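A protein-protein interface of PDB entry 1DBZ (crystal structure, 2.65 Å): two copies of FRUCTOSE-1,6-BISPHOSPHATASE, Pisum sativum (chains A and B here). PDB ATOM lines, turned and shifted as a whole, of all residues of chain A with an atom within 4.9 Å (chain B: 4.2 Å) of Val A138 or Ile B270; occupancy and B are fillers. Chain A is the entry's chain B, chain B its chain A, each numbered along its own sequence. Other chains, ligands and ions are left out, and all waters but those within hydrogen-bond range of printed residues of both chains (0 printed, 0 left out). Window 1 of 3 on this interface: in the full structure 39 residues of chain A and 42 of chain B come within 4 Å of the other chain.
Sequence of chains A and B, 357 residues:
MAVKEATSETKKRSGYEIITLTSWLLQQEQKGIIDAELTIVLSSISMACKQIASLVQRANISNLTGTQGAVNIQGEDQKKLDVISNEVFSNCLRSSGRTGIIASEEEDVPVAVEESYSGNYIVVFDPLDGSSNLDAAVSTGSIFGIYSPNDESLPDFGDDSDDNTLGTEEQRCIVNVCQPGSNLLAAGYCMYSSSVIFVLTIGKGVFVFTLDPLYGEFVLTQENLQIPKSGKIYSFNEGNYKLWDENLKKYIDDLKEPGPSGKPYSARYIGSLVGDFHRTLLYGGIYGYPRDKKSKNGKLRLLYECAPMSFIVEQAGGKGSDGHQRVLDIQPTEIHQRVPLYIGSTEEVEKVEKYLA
Of the printed residues of chain B, Val A138 touches Met B191, Ser B193, Ser B194 and Ile B270. Printed residues of chain B within 4 Å of Ser A193: Val B138, Ser B193 and Ser B194. Of the printed residues of chain B, Arg A268 touches Tyr B269, Ile B270 and Gly B271. Of the printed residues of chain B, Tyr A269 touches Tyr B269 (2.8 Å). Printed residues of chain A within 4 Å of Ser B193: Val A138 (3.3 Å), Ser A193 (2.9 Å) and Ser A194 (3.3 Å). Of the printed residues of chain A, Ser B194 touches Val A138, Tyr A192, Ser A193 and Ser A194. Of the printed residues of chain A, Ile B270 touches Val A138 (3.5 Å) and Arg A268 (3.4 Å). Asp B276 touches none of the printed residues of chain A. Arg B279 touches none of the printed residues of chain A. The nearest residue of chain A that does not touch Ile B270 is Tyr A269 (4.2 Å).
Val A138 touches Met B191 (CG1 to SD, 3.998 Å). Val A138 touches Ile B270. CB of Ser B194 touches O of Tyr A192, 3.0 Å away. Ser A193 touches Val B138 (CB to O, 3.2 Å). Ser B139 touches Ser A194. N of Ser A194 touches C of Ser B193, at 3.3 Å. Ser A194 touches Ser B194 (N to N, 3.7 Å). Ile B270 touches Arg A268. Arg A268 touches Gly B271. Ile A270 touches Val B138 (CD1 to CG2, 3.6 Å).
OG of Ser B139 is in hydrogen-bond range of OG of Ser B272. N of Ile B270 lies within hydrogen-bond range of OD1 of Asp B276, at 2.7 Å. N of Gly B271 is in hydrogen-bond range of OD2 of Asp B276 (3.0 Å). The backbone carbonyl oxygen of Thr A140 lies within hydrogen-bond range of the backbone NH of Tyr A192, 3.1 Å away.
The backbone NH (N) of Ser A194 lies within hydrogen-bond range of the backbone carbonyl oxygen (O) of Val B138, 2.8 Å away. The backbone NH (N) of Ser B194 sits at hydrogen-bond distance from the backbone carbonyl oxygen (O) of Val A138 (3.0 Å). O of Ser A193 lies close to N of Ser B194. The backbone NH (N) of Tyr B269 sits at hydrogen-bond distance from the backbone carbonyl oxygen (O) of Tyr A269 (2.8 Å). The backbone carbonyl oxygen of Ser A193 lies close to the backbone carbonyl oxygen of Ser B193 (2.9 Å).
Hydrophobic or aromatic side chains of chain B within 4 Å of the printed part of chain A: Val B138, Met B191, Tyr B269 and Ile B270. Of the 11 printed residues of chain A, 7 touch a printed residue of chain B. Along chain A the printed residues that touch a printed residue of chain B span positions 138 to 270. Among the printed residues, 17 pairs touch across the chains. Among the printed residues, no Asp or Glu carboxylate lies within 4 Å of a Lys or Arg side-chain nitrogen of the other chain.
Ser A193 touches Ser B194, and with the chains exchanged Ser A194 touches Ser B193. Ser A194 touches Ser B139, but with the chains exchanged Ser A139 does not touch Ser B194 (4.03 Å). Ser A194 touches its own counterpart, Ser B194. Tyr B269 touches its own counterpart, Tyr A269.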
ATOM      1  N   ALA A 136      -1.804  23.927  -3.175  1.00  0.00           N
ATOM      2  CA  ALA A 136      -2.539  23.749  -4.422  1.00  0.00           C
ATOM      3  C   ALA A 136      -2.604  25.046  -5.245  1.00  0.00           C
ATOM      4  O   ALA A 136      -3.402  25.168  -6.183  1.00  0.00           O
ATOM      5  CB  ALA A 136      -3.930  23.242  -4.122  1.00  0.00           C
ATOM      6  N   ALA A 137      -1.718  25.982  -4.920  1.00  0.00           N
ATOM      7  CA  ALA A 137      -1.666  27.268  -5.584  1.00  0.00           C
ATOM      8  C   ALA A 137      -1.467  27.189  -7.101  1.00  0.00           C
ATOM      9  O   ALA A 137      -2.090  27.950  -7.859  1.00  0.00           O
ATOM     10  CB  ALA A 137      -0.581  28.118  -4.959  1.00  0.00           C
ATOM     11  N   VAL A 138      -0.614  26.268  -7.544  1.00  0.00           N
ATOM     12  CA  VAL A 138      -0.330  26.111  -8.976  1.00  0.00           C
ATOM     13  C   VAL A 138      -0.651  24.725  -9.539  1.00  0.00           C
ATOM     14  O   VAL A 138      -0.779  24.568 -10.747  1.00  0.00           O
ATOM     15  CB  VAL A 138       1.153  26.453  -9.307  1.00  0.00           C
ATOM     16  CG1 VAL A 138       1.409  27.907  -9.104  1.00  0.00           C
ATOM     17  CG2 VAL A 138       2.101  25.653  -8.428  1.00  0.00           C
ATOM     18  N   SER A 139      -0.744  23.720  -8.671  1.00  0.00           N
ATOM     19  CA  SER A 139      -1.041  22.364  -9.110  1.00  0.00           C
ATOM     20  C   SER A 139      -1.592  21.486  -7.992  1.00  0.00           C
ATOM     21  O   SER A 139      -1.457  21.788  -6.814  1.00  0.00           O
ATOM     22  CB  SER A 139       0.209  21.701  -9.703  1.00  0.00           C
ATOM     23  OG  SER A 139       1.020  21.147  -8.687  1.00  0.00           O
ATOM     24  N   THR A 140      -2.253  20.413  -8.396  1.00  0.00           N
ATOM     25  CA  THR A 140      -2.815  19.430  -7.489  1.00  0.00           C
ATOM     26  C   THR A 140      -3.070  18.204  -8.384  1.00  0.00           C
ATOM     27  O   THR A 140      -2.641  18.187  -9.544  1.00  0.00           O
ATOM     28  CB  THR A 140      -4.087  19.969  -6.763  1.00  0.00           C
ATOM     29  OG1 THR A 140      -4.533  19.023  -5.790  1.00  0.00           O
ATOM     30  CG2 THR A 140      -5.198  20.247  -7.726  1.00  0.00           C
ATOM     31  N   TYR A 192      -3.284  18.205 -12.539  1.00  0.00           N
ATOM     32  CA  TYR A 192      -3.971  19.385 -13.008  1.00  0.00           C
ATOM     33  C   TYR A 192      -3.034  20.587 -12.805  1.00  0.00           C
ATOM     34  O   TYR A 192      -2.934  21.126 -11.705  1.00  0.00           O
ATOM     35  CB  TYR A 192      -5.246  19.609 -12.214  1.00  0.00           C
ATOM     36  CG  TYR A 192      -6.063  18.377 -12.031  1.00  0.00           C
ATOM     37  CD1 TYR A 192      -6.713  17.801 -13.093  1.00  0.00           C
ATOM     38  CD2 TYR A 192      -6.197  17.798 -10.788  1.00  0.00           C
ATOM     39  CE1 TYR A 192      -7.482  16.663 -12.926  1.00  0.00           C
ATOM     40  CE2 TYR A 192      -6.962  16.666 -10.600  1.00  0.00           C
ATOM     41  CZ  TYR A 192      -7.603  16.102 -11.677  1.00  0.00           C
ATOM     42  OH  TYR A 192      -8.340  14.948 -11.519  1.00  0.00           O
ATOM     43  N   SER A 193      -2.311  20.979 -13.846  1.00  0.00           N
ATOM     44  CA  SER A 193      -1.418  22.126 -13.743  1.00  0.00           C
ATOM     45  C   SER A 193      -1.523  22.962 -15.019  1.00  0.00           C
ATOM     46  O   SER A 193      -2.602  23.053 -15.605  1.00  0.00           O
ATOM     47  CB  SER A 193       0.012  21.656 -13.508  1.00  0.00           C
ATOM     48  OG  SER A 193       0.461  20.901 -14.604  1.00  0.00           O
ATOM     49  N   SER A 194      -0.426  23.579 -15.454  1.00  0.00           N
ATOM     50  CA  SER A 194      -0.465  24.373 -16.684  1.00  0.00           C
ATOM     51  C   SER A 194      -0.919  23.465 -17.832  1.00  0.00           C
ATOM     52  O   SER A 194      -1.264  23.920 -18.912  1.00  0.00           O
ATOM     53  CB  SER A 194       0.911  24.975 -17.001  1.00  0.00           C
ATOM     54  OG  SER A 194       1.785  24.019 -17.560  1.00  0.00           O
ATOM     55  N   ARG A 268      13.829  22.067  -5.677  1.00  0.00           N
ATOM     56  CA  ARG A 268      12.509  22.351  -6.251  1.00  0.00           C
ATOM     57  C   ARG A 268      11.463  21.660  -5.377  1.00  0.00           C
ATOM     58  O   ARG A 268      11.476  20.444  -5.236  1.00  0.00           O
ATOM     59  CB  ARG A 268      12.402  21.792  -7.673  1.00  0.00           C
ATOM     60  CG  ARG A 268      13.253  22.478  -8.714  1.00  0.00           C
ATOM     61  CD  ARG A 268      12.819  23.918  -8.906  1.00  0.00           C
ATOM     62  NE  ARG A 268      13.593  24.559  -9.965  1.00  0.00           N
ATOM     63  CZ  ARG A 268      14.838  25.008  -9.822  1.00  0.00           C
ATOM     64  NH1 ARG A 268      15.460  24.893  -8.663  1.00  0.00           N
ATOM     65  NH2 ARG A 268      15.470  25.570 -10.835  1.00  0.00           N
ATOM     66  N   TYR A 269      10.544  22.430  -4.809  1.00  0.00           N
ATOM     67  CA  TYR A 269       9.502  21.885  -3.952  1.00  0.00           C
ATOM     68  C   TYR A 269       8.238  22.719  -4.132  1.00  0.00           C
ATOM     69  O   TYR A 269       8.130  23.814  -3.587  1.00  0.00           O
ATOM     70  CB  TYR A 269       9.943  21.954  -2.496  1.00  0.00           C
ATOM     71  CG  TYR A 269       9.096  21.136  -1.563  1.00  0.00           C
ATOM     72  CD1 TYR A 269       9.159  19.752  -1.582  1.00  0.00           C
ATOM     73  CD2 TYR A 269       8.214  21.731  -0.695  1.00  0.00           C
ATOM     74  CE1 TYR A 269       8.371  18.985  -0.756  1.00  0.00           C
ATOM     75  CE2 TYR A 269       7.412  20.965   0.141  1.00  0.00           C
ATOM     76  CZ  TYR A 269       7.507  19.601   0.094  1.00  0.00           C
ATOM     77  OH  TYR A 269       6.767  18.825   0.954  1.00  0.00           O
ATOM     78  N   ILE A 270       7.274  22.182  -4.871  1.00  0.00           N
ATOM     79  CA  ILE A 270       6.034  22.882  -5.152  1.00  0.00           C
ATOM     80  C   ILE A 270       5.149  22.851  -3.942  1.00  0.00           C
ATOM     81  O   ILE A 270       4.550  23.857  -3.553  1.00  0.00           O
ATOM     82  CB  ILE A 270       5.315  22.221  -6.322  1.00  0.00           C
ATOM     83  CG1 ILE A 270       6.207  22.220  -7.555  1.00  0.00           C
ATOM     84  CG2 ILE A 270       4.044  22.941  -6.625  1.00  0.00           C
ATOM     85  CD1 ILE A 270       5.706  21.341  -8.625  1.00  0.00           C
ATOM     86  N   VAL B 138       4.885  22.597 -14.151  1.00  0.00           N
ATOM     87  CA  VAL B 138       3.517  22.777 -13.665  1.00  0.00           C
ATOM     88  C   VAL B 138       2.941  24.180 -13.899  1.00  0.00           C
ATOM     89  O   VAL B 138       1.725  24.362 -13.898  1.00  0.00           O
ATOM     90  CB  VAL B 138       3.373  22.428 -12.150  1.00  0.00           C
ATOM     91  CG1 VAL B 138       3.601  20.943 -11.907  1.00  0.00           C
ATOM     92  CG2 VAL B 138       4.344  23.240 -11.322  1.00  0.00           C
ATOM     93  N   SER B 139       3.806  25.170 -14.095  1.00  0.00           N
ATOM     94  CA  SER B 139       3.333  26.520 -14.320  1.00  0.00           C
ATOM     95  C   SER B 139       4.368  27.384 -15.010  1.00  0.00           C
ATOM     96  O   SER B 139       5.550  27.081 -15.005  1.00  0.00           O
ATOM     97  CB  SER B 139       2.971  27.172 -13.001  1.00  0.00           C
ATOM     98  OG  SER B 139       4.149  27.646 -12.377  1.00  0.00           O
ATOM     99  N   MET B 191      -0.791  34.051 -15.294  1.00  0.00           N
ATOM    100  CA  MET B 191      -0.209  32.801 -14.916  1.00  0.00           C
ATOM    101  C   MET B 191      -0.917  31.644 -15.578  1.00  0.00           C
ATOM    102  O   MET B 191      -2.140  31.575 -15.548  1.00  0.00           O
ATOM    103  CB  MET B 191      -0.268  32.639 -13.405  1.00  0.00           C
ATOM    104  CG  MET B 191       0.358  31.355 -12.904  1.00  0.00           C
ATOM    105  SD  MET B 191       0.256  31.146 -11.144  1.00  0.00           S
ATOM    106  CE  MET B 191      -1.519  30.845 -10.966  1.00  0.00           C
ATOM    107  N   SER B 193      -1.337  27.924 -15.062  1.00  0.00           N
ATOM    108  CA  SER B 193      -1.092  26.760 -14.235  1.00  0.00           C
ATOM    109  C   SER B 193      -2.373  25.961 -14.162  1.00  0.00           C
ATOM    110  O   SER B 193      -3.108  25.905 -15.146  1.00  0.00           O
ATOM    111  CB  SER B 193      -0.600  27.172 -12.840  1.00  0.00           C
ATOM    112  OG  SER B 193      -1.582  27.896 -12.143  1.00  0.00           O
ATOM    113  N   SER B 194      -2.643  25.341 -13.011  1.00  0.00           N
ATOM    114  CA  SER B 194      -3.854  24.547 -12.837  1.00  0.00           C
ATOM    115  C   SER B 194      -5.052  25.447 -13.092  1.00  0.00           C
ATOM    116  O   SER B 194      -6.171  24.978 -13.288  1.00  0.00           O
ATOM    117  CB  SER B 194      -3.931  23.948 -11.430  1.00  0.00           C
ATOM    118  OG  SER B 194      -4.300  24.905 -10.446  1.00  0.00           O
ATOM    119  N   TYR B 269       9.221  26.430  -3.331  1.00  0.00           N
ATOM    120  CA  TYR B 269       9.922  27.004  -4.478  1.00  0.00           C
ATOM    121  C   TYR B 269       9.589  26.204  -5.730  1.00  0.00           C
ATOM    122  O   TYR B 269      10.110  25.115  -5.939  1.00  0.00           O
ATOM    123  CB  TYR B 269      11.429  26.998  -4.232  1.00  0.00           C
ATOM    124  CG  TYR B 269      12.230  27.794  -5.229  1.00  0.00           C
ATOM    125  CD1 TYR B 269      12.210  29.178  -5.190  1.00  0.00           C
ATOM    126  CD2 TYR B 269      13.010  27.168  -6.196  1.00  0.00           C
ATOM    127  CE1 TYR B 269      12.932  29.920  -6.069  1.00  0.00           C
ATOM    128  CE2 TYR B 269      13.750  27.910  -7.091  1.00  0.00           C
ATOM    129  CZ  TYR B 269      13.694  29.293  -7.006  1.00  0.00           C
ATOM    130  OH  TYR B 269      14.405  30.101  -7.859  1.00  0.00           O
ATOM    131  N   ILE B 270       8.730  26.768  -6.567  1.00  0.00           N
ATOM    132  CA  ILE B 270       8.314  26.103  -7.789  1.00  0.00           C
ATOM    133  C   ILE B 270       9.402  26.086  -8.852  1.00  0.00           C
ATOM    134  O   ILE B 270       9.654  25.056  -9.482  1.00  0.00           O
ATOM    135  CB  ILE B 270       7.053  26.764  -8.358  1.00  0.00           C
ATOM    136  CG1 ILE B 270       5.960  26.765  -7.301  1.00  0.00           C
ATOM    137  CG2 ILE B 270       6.582  26.023  -9.586  1.00  0.00           C
ATOM    138  CD1 ILE B 270       4.847  27.645  -7.647  1.00  0.00           C
ATOM    139  N   GLY B 271      10.088  27.214  -8.982  1.00  0.00           N
ATOM    140  CA  GLY B 271      11.126  27.377  -9.984  1.00  0.00           C
ATOM    141  C   GLY B 271      10.650  28.408 -11.006  1.00  0.00           C
ATOM    142  O   GLY B 271      11.444  28.987 -11.754  1.00  0.00           O
ATOM    143  N   SER B 272       9.336  28.648 -10.998  1.00  0.00           N
ATOM    144  CA  SER B 272       8.646  29.596 -11.870  1.00  0.00           C
ATOM    145  C   SER B 272       8.484  30.930 -11.159  1.00  0.00           C
ATOM    146  O   SER B 272       7.864  31.003 -10.102  1.00  0.00           O
ATOM    147  CB  SER B 272       7.267  29.035 -12.196  1.00  0.00           C
ATOM    148  OG  SER B 272       6.462  29.990 -12.853  1.00  0.00           O
ATOM    149  N   GLY B 275       4.809  31.808 -10.934  1.00  0.00           N
ATOM    150  CA  GLY B 275       4.187  30.894  -9.982  1.00  0.00           C
ATOM    151  C   GLY B 275       4.578  31.171  -8.530  1.00  0.00           C
ATOM    152  O   GLY B 275       3.736  31.211  -7.632  1.00  0.00           O
ATOM    153  N   ASP B 276       5.869  31.360  -8.295  1.00  0.00           N
ATOM    154  CA  ASP B 276       6.352  31.650  -6.960  1.00  0.00           C
ATOM    155  C   ASP B 276       5.909  33.049  -6.542  1.00  0.00           C
ATOM    156  O   ASP B 276       5.504  33.260  -5.411  1.00  0.00           O
ATOM    157  CB  ASP B 276       7.872  31.527  -6.907  1.00  0.00           C
ATOM    158  CG  ASP B 276       8.357  30.064  -6.890  1.00  0.00           C
ATOM    159  OD1 ASP B 276       7.834  29.228  -6.114  1.00  0.00           O
ATOM    160  OD2 ASP B 276       9.299  29.752  -7.633  1.00  0.00           O
ATOM    161  N   ARG B 279       1.925  33.042  -5.545  1.00  0.00           N
ATOM    162  CA  ARG B 279       1.633  32.437  -4.258  1.00  0.00           C
ATOM    163  C   ARG B 279       2.068  33.363  -3.137  1.00  0.00           C
ATOM    164  O   ARG B 279       1.456  33.376  -2.081  1.00  0.00           O
ATOM    165  CB  ARG B 279       2.371  31.109  -4.129  1.00  0.00           C
ATOM    166  CG  ARG B 279       2.111  30.306  -2.845  1.00  0.00           C
ATOM    167  CD  ARG B 279       3.222  29.275  -2.645  1.00  0.00           C
ATOM    168  NE  ARG B 279       4.505  29.968  -2.506  1.00  0.00           N
ATOM    169  CZ  ARG B 279       5.610  29.671  -3.178  1.00  0.00           C
ATOM    170  NH1 ARG B 279       5.618  28.668  -4.046  1.00  0.00           N
ATOM    171  NH2 ARG B 279       6.690  30.427  -3.028  1.00  0.00           N
